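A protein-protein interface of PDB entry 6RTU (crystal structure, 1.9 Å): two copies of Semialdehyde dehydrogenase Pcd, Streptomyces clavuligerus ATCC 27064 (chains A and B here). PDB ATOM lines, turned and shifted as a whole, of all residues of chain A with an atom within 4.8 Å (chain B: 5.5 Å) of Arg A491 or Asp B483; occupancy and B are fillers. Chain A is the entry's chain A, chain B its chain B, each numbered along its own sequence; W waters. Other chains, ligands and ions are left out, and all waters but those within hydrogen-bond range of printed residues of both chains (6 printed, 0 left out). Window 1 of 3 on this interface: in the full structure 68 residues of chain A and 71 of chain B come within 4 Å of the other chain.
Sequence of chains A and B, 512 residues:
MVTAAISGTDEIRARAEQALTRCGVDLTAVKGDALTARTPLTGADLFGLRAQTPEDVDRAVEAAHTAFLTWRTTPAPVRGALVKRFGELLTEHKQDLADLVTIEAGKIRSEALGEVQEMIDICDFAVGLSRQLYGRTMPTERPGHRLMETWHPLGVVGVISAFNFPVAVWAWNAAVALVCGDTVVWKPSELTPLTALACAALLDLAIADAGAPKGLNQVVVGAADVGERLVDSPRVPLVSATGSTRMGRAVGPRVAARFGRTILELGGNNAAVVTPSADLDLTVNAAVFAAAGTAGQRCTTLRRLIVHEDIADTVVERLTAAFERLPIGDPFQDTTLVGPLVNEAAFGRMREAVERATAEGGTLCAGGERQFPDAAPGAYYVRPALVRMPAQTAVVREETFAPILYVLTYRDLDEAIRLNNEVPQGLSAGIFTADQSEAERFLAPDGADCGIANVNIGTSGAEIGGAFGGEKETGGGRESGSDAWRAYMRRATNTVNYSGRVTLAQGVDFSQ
The guanidinium group (NH1) of Arg A136 sits at hydrogen-bond distance from the side-chain hydroxyl (OG) of Ser B482 (3.2 Å).
NH1 of Arg A136 lies within salt-bridge range of OD2 of Asp B483 (3.96 Å).
The side-chain carboxylate of Glu A149 sits at hydrogen-bond distance from the side-chain hydroxyl of Ser B482.
The guanidinium group (NH2) of Arg B478 sits at hydrogen-bond distance from the backbone carbonyl oxygen (O) of Arg A491.
The side-chain carboxylate of Asp B483 lies within salt-bridge range of the guanidinium group of Arg A491 (3.0 Å).
O of Gly B451 lies within hydrogen-bond range of N of Thr A493, 2.9 Å away.
The backbone carbonyl oxygen (O) of Ala B467 sits at hydrogen-bond distance from the side-chain hydroxyl (OG1) of Thr A493 (3.0 Å).
The backbone carbonyl oxygen of Arg A136 lies within hydrogen-bond range of the backbone NH of Glu A149, 2.8 Å away.
The side-chain carboxylate of Glu A149 lies within hydrogen-bond range of the indole nitrogen of Trp A151, at 3.5 Å.
OE2 of Glu A149 is in salt-bridge range of NH1 of Arg A491 (2.9 Å).
The backbone NH (N) of Ala A492 is in hydrogen-bond range of the backbone carbonyl oxygen (O) of Thr A150, 2.8 Å away.
The guanidinium group of Arg B478 lies within salt-bridge range of the side-chain carboxylate of Glu B471 (3.0 Å).
Among the printed residues, pairs that only touch across the chains: Arg A490 with Glu B471, Arg A491 with Gly B451, Arg A491 with Ala B467, Arg A491 with Ser B482 and Ala A492 with Gly B451.
Of the printed residues of chain B, Arg A136 touches Ser B482 (3.2 Å) and Asp B483 (3.6 Å).
Of the printed residues of chain B, Glu A149 touches Ser B482 (2.9 Å).
Thr A150 touches none of the printed residues of chain B.
Of the printed residues of chain B, Arg A490 touches Glu B471 (3.9 Å).
Printed residues of chain A within 4 Å of Ala B467: Arg A491 and Thr A493.
Of the printed residues of chain A, Arg B478 touches Arg A491 (2.9 Å).
Printed residues of chain A within 4 Å of Asp B483: Arg A136 (3.6 Å) and Arg A491 (3.0 Å).
The nearest printed residue of chain A that does not touch Asp B483 is Glu A149 (4.9 Å).
Hydrophobic or aromatic side chains of chain B within 4 Å of the printed part of chain A: Ala B467.
No position is printed for both chains.
Water W1 lies within hydrogen-bond range of OE2 of Glu A149, N of Ala B467 and OG1 of Thr A493.
Water W2 bridges O of Asp B483 (2.8 Å) and NH2 of Arg A491 (3.1 Å).
Water W5 lies within hydrogen-bond range of O of Cys B450, O of Arg A491 and NH1 of Arg A490.
Water W3 lies within hydrogen-bond range of the backbone carbonyl oxygen (O) of Cys B450 (2.8 Å) and the guanidinium group (NH1) of Arg A490 (3.5 Å).
Water W4 bridges OD2 of Asp B483 and OE1 of Glu A149.
Water W6 lies within hydrogen-bond range of the guanidinium group of Arg B478 (2.8 Å), the side-chain hydroxyl of Thr A493 (2.8 Å) and the backbone carbonyl oxygen of Gly B451 (2.9 Å).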
ATOM      1  N   ARG A 136     -11.921  -8.013 -27.723  1.00  0.00           N
ATOM      2  CA  ARG A 136     -12.516  -6.846 -28.362  1.00  0.00           C
ATOM      3  C   ARG A 136     -11.654  -6.350 -29.518  1.00  0.00           C
ATOM      4  O   ARG A 136     -10.442  -6.570 -29.554  1.00  0.00           O
ATOM      5  CB  ARG A 136     -12.718  -5.710 -27.344  1.00  0.00           C
ATOM      6  CG  ARG A 136     -13.879  -5.990 -26.393  1.00  0.00           C
ATOM      7  CD  ARG A 136     -13.918  -5.082 -25.175  1.00  0.00           C
ATOM      8  NE  ARG A 136     -15.232  -5.186 -24.527  1.00  0.00           N
ATOM      9  CZ  ARG A 136     -15.612  -4.491 -23.456  1.00  0.00           C
ATOM     10  NH1 ARG A 136     -14.774  -3.637 -22.875  1.00  0.00           N
ATOM     11  NH2 ARG A 136     -16.828  -4.662 -22.954  1.00  0.00           N
ATOM     12  N   GLU A 149      -7.925  -6.431 -28.388  1.00  0.00           N
ATOM     13  CA  GLU A 149      -7.653  -7.143 -27.151  1.00  0.00           C
ATOM     14  C   GLU A 149      -7.947  -8.623 -27.375  1.00  0.00           C
ATOM     15  O   GLU A 149      -9.040  -8.978 -27.839  1.00  0.00           O
ATOM     16  CB  GLU A 149      -8.514  -6.556 -26.027  1.00  0.00           C
ATOM     17  CG  GLU A 149      -8.458  -7.263 -24.707  1.00  0.00           C
ATOM     18  CD  GLU A 149      -9.539  -6.739 -23.760  1.00  0.00           C
ATOM     19  OE1 GLU A 149     -10.572  -7.434 -23.583  1.00  0.00           O
ATOM     20  OE2 GLU A 149      -9.356  -5.620 -23.227  1.00  0.00           O
ATOM     21  N   THR A 150      -6.972  -9.479 -27.079  1.00  0.00           N
ATOM     22  CA  THR A 150      -7.100 -10.923 -27.260  1.00  0.00           C
ATOM     23  C   THR A 150      -6.911 -11.637 -25.922  1.00  0.00           C
ATOM     24  O   THR A 150      -6.361 -11.077 -24.972  1.00  0.00           O
ATOM     25  CB  THR A 150      -6.081 -11.458 -28.287  1.00  0.00           C
ATOM     26  OG1 THR A 150      -4.760 -11.049 -27.905  1.00  0.00           O
ATOM     27  CG2 THR A 150      -6.391 -10.918 -29.691  1.00  0.00           C
ATOM     28  N   TRP A 151      -7.407 -12.879 -25.842  1.00  0.00           N
ATOM     29  CA  TRP A 151      -7.290 -13.704 -24.644  1.00  0.00           C
ATOM     30  C   TRP A 151      -6.514 -14.970 -24.987  1.00  0.00           C
ATOM     31  O   TRP A 151      -6.794 -15.630 -26.001  1.00  0.00           O
ATOM     32  CB  TRP A 151      -8.679 -14.033 -24.058  1.00  0.00           C
ATOM     33  CG  TRP A 151      -9.328 -12.813 -23.492  1.00  0.00           C
ATOM     34  CD1 TRP A 151     -10.114 -11.913 -24.162  1.00  0.00           C
ATOM     35  CD2 TRP A 151      -9.202 -12.317 -22.154  1.00  0.00           C
ATOM     36  NE1 TRP A 151     -10.490 -10.890 -23.315  1.00  0.00           N
ATOM     37  CE2 TRP A 151      -9.957 -11.126 -22.075  1.00  0.00           C
ATOM     38  CE3 TRP A 151      -8.533 -12.770 -21.008  1.00  0.00           C
ATOM     39  CZ2 TRP A 151     -10.057 -10.388 -20.910  1.00  0.00           C
ATOM     40  CZ3 TRP A 151      -8.645 -12.039 -19.845  1.00  0.00           C
ATOM     41  CH2 TRP A 151      -9.396 -10.857 -19.805  1.00  0.00           C
ATOM     42  N   MET A 489      -7.519 -17.091 -18.229  1.00  0.00           N
ATOM     43  CA  MET A 489      -6.744 -16.692 -19.393  1.00  0.00           C
ATOM     44  C   MET A 489      -6.014 -15.388 -19.085  1.00  0.00           C
ATOM     45  O   MET A 489      -6.257 -14.742 -18.061  1.00  0.00           O
ATOM     46  CB  MET A 489      -7.650 -16.544 -20.625  1.00  0.00           C
ATOM     47  CG  MET A 489      -8.485 -17.812 -20.920  1.00  0.00           C
ATOM     48  SD  MET A 489      -9.405 -17.810 -22.481  1.00  0.00           S
ATOM     49  CE  MET A 489      -8.110 -18.052 -23.718  1.00  0.00           C
ATOM     50  N   ARG A 490      -5.096 -14.999 -19.967  1.00  0.00           N
ATOM     51  CA  ARG A 490      -4.418 -13.719 -19.838  1.00  0.00           C
ATOM     52  C   ARG A 490      -4.819 -12.789 -20.978  1.00  0.00           C
ATOM     53  O   ARG A 490      -4.893 -13.206 -22.137  1.00  0.00           O
ATOM     54  CB  ARG A 490      -2.893 -13.883 -19.794  1.00  0.00           C
ATOM     55  CG  ARG A 490      -2.261 -14.636 -20.932  1.00  0.00           C
ATOM     56  CD  ARG A 490      -0.723 -14.578 -20.828  1.00  0.00           C
ATOM     57  NE  ARG A 490      -0.110 -15.466 -21.812  1.00  0.00           N
ATOM     58  CZ  ARG A 490       0.059 -15.157 -23.097  1.00  0.00           C
ATOM     59  NH1 ARG A 490      -0.329 -13.983 -23.567  1.00  0.00           N
ATOM     60  NH2 ARG A 490       0.606 -16.034 -23.917  1.00  0.00           N
ATOM     61  N   ARG A 491      -5.095 -11.533 -20.626  1.00  0.00           N
ATOM     62  CA  ARG A 491      -5.474 -10.500 -21.589  1.00  0.00           C
ATOM     63  C   ARG A 491      -4.223  -9.950 -22.267  1.00  0.00           C
ATOM     64  O   ARG A 491      -3.192  -9.771 -21.618  1.00  0.00           O
ATOM     65  CB  ARG A 491      -6.220  -9.374 -20.857  1.00  0.00           C
ATOM     66  CG  ARG A 491      -6.852  -8.293 -21.731  1.00  0.00           C
ATOM     67  CD  ARG A 491      -7.140  -6.987 -20.928  1.00  0.00           C
ATOM     68  NE  ARG A 491      -7.915  -7.215 -19.702  1.00  0.00           N
ATOM     69  CZ  ARG A 491      -9.195  -6.880 -19.526  1.00  0.00           C
ATOM     70  NH1 ARG A 491      -9.891  -6.284 -20.493  1.00  0.00           N
ATOM     71  NH2 ARG A 491      -9.785  -7.139 -18.365  1.00  0.00           N
ATOM     72  N   ALA A 492      -4.292  -9.733 -23.582  1.00  0.00           N
ATOM     73  CA  ALA A 492      -3.252  -9.002 -24.304  1.00  0.00           C
ATOM     74  C   ALA A 492      -3.879  -7.857 -25.080  1.00  0.00           C
ATOM     75  O   ALA A 492      -4.948  -8.014 -25.682  1.00  0.00           O
ATOM     76  CB  ALA A 492      -2.458  -9.895 -25.278  1.00  0.00           C
ATOM     77  N   THR A 493      -3.219  -6.701 -25.039  1.00  0.00           N
ATOM     78  CA  THR A 493      -3.607  -5.529 -25.816  1.00  0.00           C
ATOM     79  C   THR A 493      -2.636  -5.390 -26.984  1.00  0.00           C
ATOM     80  O   THR A 493      -1.429  -5.226 -26.765  1.00  0.00           O
ATOM     81  CB  THR A 493      -3.563  -4.278 -24.932  1.00  0.00           C
ATOM     82  OG1 THR A 493      -4.430  -4.437 -23.797  1.00  0.00           O
ATOM     83  CG2 THR A 493      -3.973  -3.024 -25.729  1.00  0.00           C
ATOM     84  N   CYS B 450       3.454 -11.117 -23.057  1.00  0.00           N
ATOM     85  CA  CYS B 450       3.293  -9.889 -22.295  1.00  0.00           C
ATOM     86  C   CYS B 450       1.852  -9.381 -22.328  1.00  0.00           C
ATOM     87  O   CYS B 450       1.029  -9.794 -23.153  1.00  0.00           O
ATOM     88  CB  CYS B 450       4.245  -8.813 -22.833  1.00  0.00           C
ATOM     89  SG  CYS B 450       6.003  -9.210 -22.639  1.00  0.00           S
ATOM     90  N   GLY B 451       1.551  -8.467 -21.402  1.00  0.00           N
ATOM     91  CA  GLY B 451       0.234  -7.851 -21.390  1.00  0.00           C
ATOM     92  C   GLY B 451      -0.024  -6.969 -22.600  1.00  0.00           C
ATOM     93  O   GLY B 451      -1.178  -6.785 -23.003  1.00  0.00           O
ATOM     94  N   ALA B 467      -6.748  -1.544 -22.127  1.00  0.00           N
ATOM     95  CA  ALA B 467      -6.353  -1.921 -20.775  1.00  0.00           C
ATOM     96  C   ALA B 467      -4.831  -1.901 -20.692  1.00  0.00           C
ATOM     97  O   ALA B 467      -4.146  -2.381 -21.599  1.00  0.00           O
ATOM     98  CB  ALA B 467      -6.904  -3.317 -20.424  1.00  0.00           C
ATOM     99  N   GLU B 471       1.993  -9.015 -17.111  1.00  0.00           N
ATOM    100  CA  GLU B 471       1.911 -10.356 -16.552  1.00  0.00           C
ATOM    101  C   GLU B 471       3.158 -10.670 -15.724  1.00  0.00           C
ATOM    102  O   GLU B 471       4.105  -9.881 -15.643  1.00  0.00           O
ATOM    103  CB  GLU B 471       1.733 -11.389 -17.675  1.00  0.00           C
ATOM    104  CG  GLU B 471       0.391 -11.302 -18.406  1.00  0.00           C
ATOM    105  CD  GLU B 471      -0.775 -11.451 -17.450  1.00  0.00           C
ATOM    106  OE1 GLU B 471      -0.866 -12.509 -16.791  1.00  0.00           O
ATOM    107  OE2 GLU B 471      -1.587 -10.504 -17.335  1.00  0.00           O
ATOM    108  N   ARG B 478      -4.695  -4.381 -14.355  1.00  0.00           N
ATOM    109  CA  ARG B 478      -5.010  -3.613 -15.554  1.00  0.00           C
ATOM    110  C   ARG B 478      -5.650  -2.291 -15.151  1.00  0.00           C
ATOM    111  O   ARG B 478      -6.510  -2.254 -14.260  1.00  0.00           O
ATOM    112  CB  ARG B 478      -5.965  -4.375 -16.498  1.00  0.00           C
ATOM    113  CG  ARG B 478      -5.353  -5.611 -17.186  1.00  0.00           C
ATOM    114  CD  ARG B 478      -4.204  -5.240 -18.147  1.00  0.00           C
ATOM    115  NE  ARG B 478      -3.729  -6.405 -18.915  1.00  0.00           N
ATOM    116  CZ  ARG B 478      -2.928  -7.348 -18.418  1.00  0.00           C
ATOM    117  NH1 ARG B 478      -2.519  -7.270 -17.154  1.00  0.00           N
ATOM    118  NH2 ARG B 478      -2.542  -8.373 -19.177  1.00  0.00           N
ATOM    119  N   GLY B 481      -8.218   1.598 -19.801  1.00  0.00           N
ATOM    120  CA  GLY B 481      -9.211   1.353 -20.828  1.00  0.00           C
ATOM    121  C   GLY B 481      -9.852  -0.028 -20.779  1.00  0.00           C
ATOM    122  O   GLY B 481      -9.709  -0.791 -19.819  1.00  0.00           O
ATOM    123  N   SER B 482     -10.571  -0.347 -21.870  1.00  0.00           N
ATOM    124  CA  SER B 482     -11.475  -1.519 -22.018  1.00  0.00           C
ATOM    125  C   SER B 482     -12.378  -1.567 -20.784  1.00  0.00           C
ATOM    126  O   SER B 482     -12.958  -0.528 -20.424  1.00  0.00           O
ATOM    127  CB  SER B 482     -10.680  -2.794 -22.299  1.00  0.00           C
ATOM    128  OG  SER B 482     -11.543  -3.857 -22.738  1.00  0.00           O
ATOM    129  N   ASP B 483     -12.546  -2.724 -20.132  1.00  0.00           N
ATOM    130  CA  ASP B 483     -13.334  -2.832 -18.904  1.00  0.00           C
ATOM    131  C   ASP B 483     -12.463  -3.003 -17.658  1.00  0.00           C
ATOM    132  O   ASP B 483     -12.814  -3.729 -16.726  1.00  0.00           O
ATOM    133  CB  ASP B 483     -14.354  -3.963 -18.990  1.00  0.00           C
ATOM    134  CG  ASP B 483     -13.758  -5.262 -19.452  1.00  0.00           C
ATOM    135  OD1 ASP B 483     -12.517  -5.407 -19.440  1.00  0.00           O
ATOM    136  OD2 ASP B 483     -14.557  -6.147 -19.819  1.00  0.00           O
ATOM    137  N   ALA B 484     -11.339  -2.291 -17.608  1.00  0.00           N
ATOM    138  CA  ALA B 484     -10.551  -2.222 -16.377  1.00  0.00           C
ATOM    139  C   ALA B 484     -11.339  -1.651 -15.198  1.00  0.00           C
ATOM    140  O   ALA B 484     -10.982  -1.928 -14.045  1.00  0.00           O
ATOM    141  CB  ALA B 484      -9.294  -1.381 -16.616  1.00  0.00           C
ATOM    142  N   TRP B 485     -12.383  -0.850 -15.463  1.00  0.00           N
ATOM    143  CA  TRP B 485     -13.243  -0.306 -14.408  1.00  0.00           C
ATOM    144  C   TRP B 485     -13.816  -1.375 -13.472  1.00  0.00           C
ATOM    145  O   TRP B 485     -14.118  -1.078 -12.305  1.00  0.00           O
ATOM    146  CB  TRP B 485     -14.393   0.511 -15.036  1.00  0.00           C
ATOM    147  CG  TRP B 485     -15.347  -0.290 -15.913  1.00  0.00           C
ATOM    148  CD1 TRP B 485     -15.313  -0.401 -17.272  1.00  0.00           C
ATOM    149  CD2 TRP B 485     -16.471  -1.077 -15.473  1.00  0.00           C
ATOM    150  NE1 TRP B 485     -16.343  -1.220 -17.708  1.00  0.00           N
ATOM    151  CE2 TRP B 485     -17.075  -1.629 -16.625  1.00  0.00           C
ATOM    152  CE3 TRP B 485     -17.039  -1.344 -14.222  1.00  0.00           C
ATOM    153  CZ2 TRP B 485     -18.196  -2.463 -16.556  1.00  0.00           C
ATOM    154  CZ3 TRP B 485     -18.153  -2.171 -14.156  1.00  0.00           C
ATOM    155  CH2 TRP B 485     -18.714  -2.722 -15.316  1.00  0.00           C
ATOM    156  N   ARG B 486     -13.941  -2.624 -13.937  1.00  0.00           N
ATOM    157  CA  ARG B 486     -14.544  -3.676 -13.118  1.00  0.00           C
ATOM    158  C   ARG B 486     -13.754  -3.938 -11.837  1.00  0.00           C
ATOM    159  O   ARG B 486     -14.330  -4.341 -10.826  1.00  0.00           O
ATOM    160  CB  ARG B 486     -14.672  -4.976 -13.930  1.00  0.00           C
ATOM    161  CG  ARG B 486     -15.630  -4.847 -15.114  1.00  0.00           C
ATOM    162  CD  ARG B 486     -15.963  -6.191 -15.763  1.00  0.00           C
ATOM    163  NE  ARG B 486     -17.312  -6.137 -16.334  1.00  0.00           N
ATOM    164  CZ  ARG B 486     -17.987  -7.193 -16.779  1.00  0.00           C
ATOM    165  NH1 ARG B 486     -17.444  -8.411 -16.735  1.00  0.00           N
ATOM    166  NH2 ARG B 486     -19.211  -7.030 -17.272  1.00  0.00           N
ATOM    167  N   ALA B 487     -12.450  -3.694 -11.848  1.00  0.00           N
ATOM    168  CA  ALA B 487     -11.652  -3.874 -10.640  1.00  0.00           C
ATOM    169  C   ALA B 487     -12.004  -2.876  -9.545  1.00  0.00           C
ATOM    170  O   ALA B 487     -11.627  -3.096  -8.384  1.00  0.00           O
ATOM    171  CB  ALA B 487     -10.166  -3.762 -10.996  1.00  0.00           C
HETATM  172  O   HOH W   1      -7.414  -3.797 -23.824  1.00  0.00           O
HETATM  173  O   HOH W   2     -11.741  -6.226 -16.165  1.00  0.00           O
HETATM  174  O   HOH W   3       0.623 -11.280 -25.515  1.00  0.00           O
HETATM  175  O   HOH W   4     -13.091  -7.037 -22.077  1.00  0.00           O
HETATM  176  O   HOH W   5      -0.953 -11.425 -22.034  1.00  0.00           O
HETATM  177  O   HOH W   6      -3.740  -6.276 -21.748  1.00  0.00           O
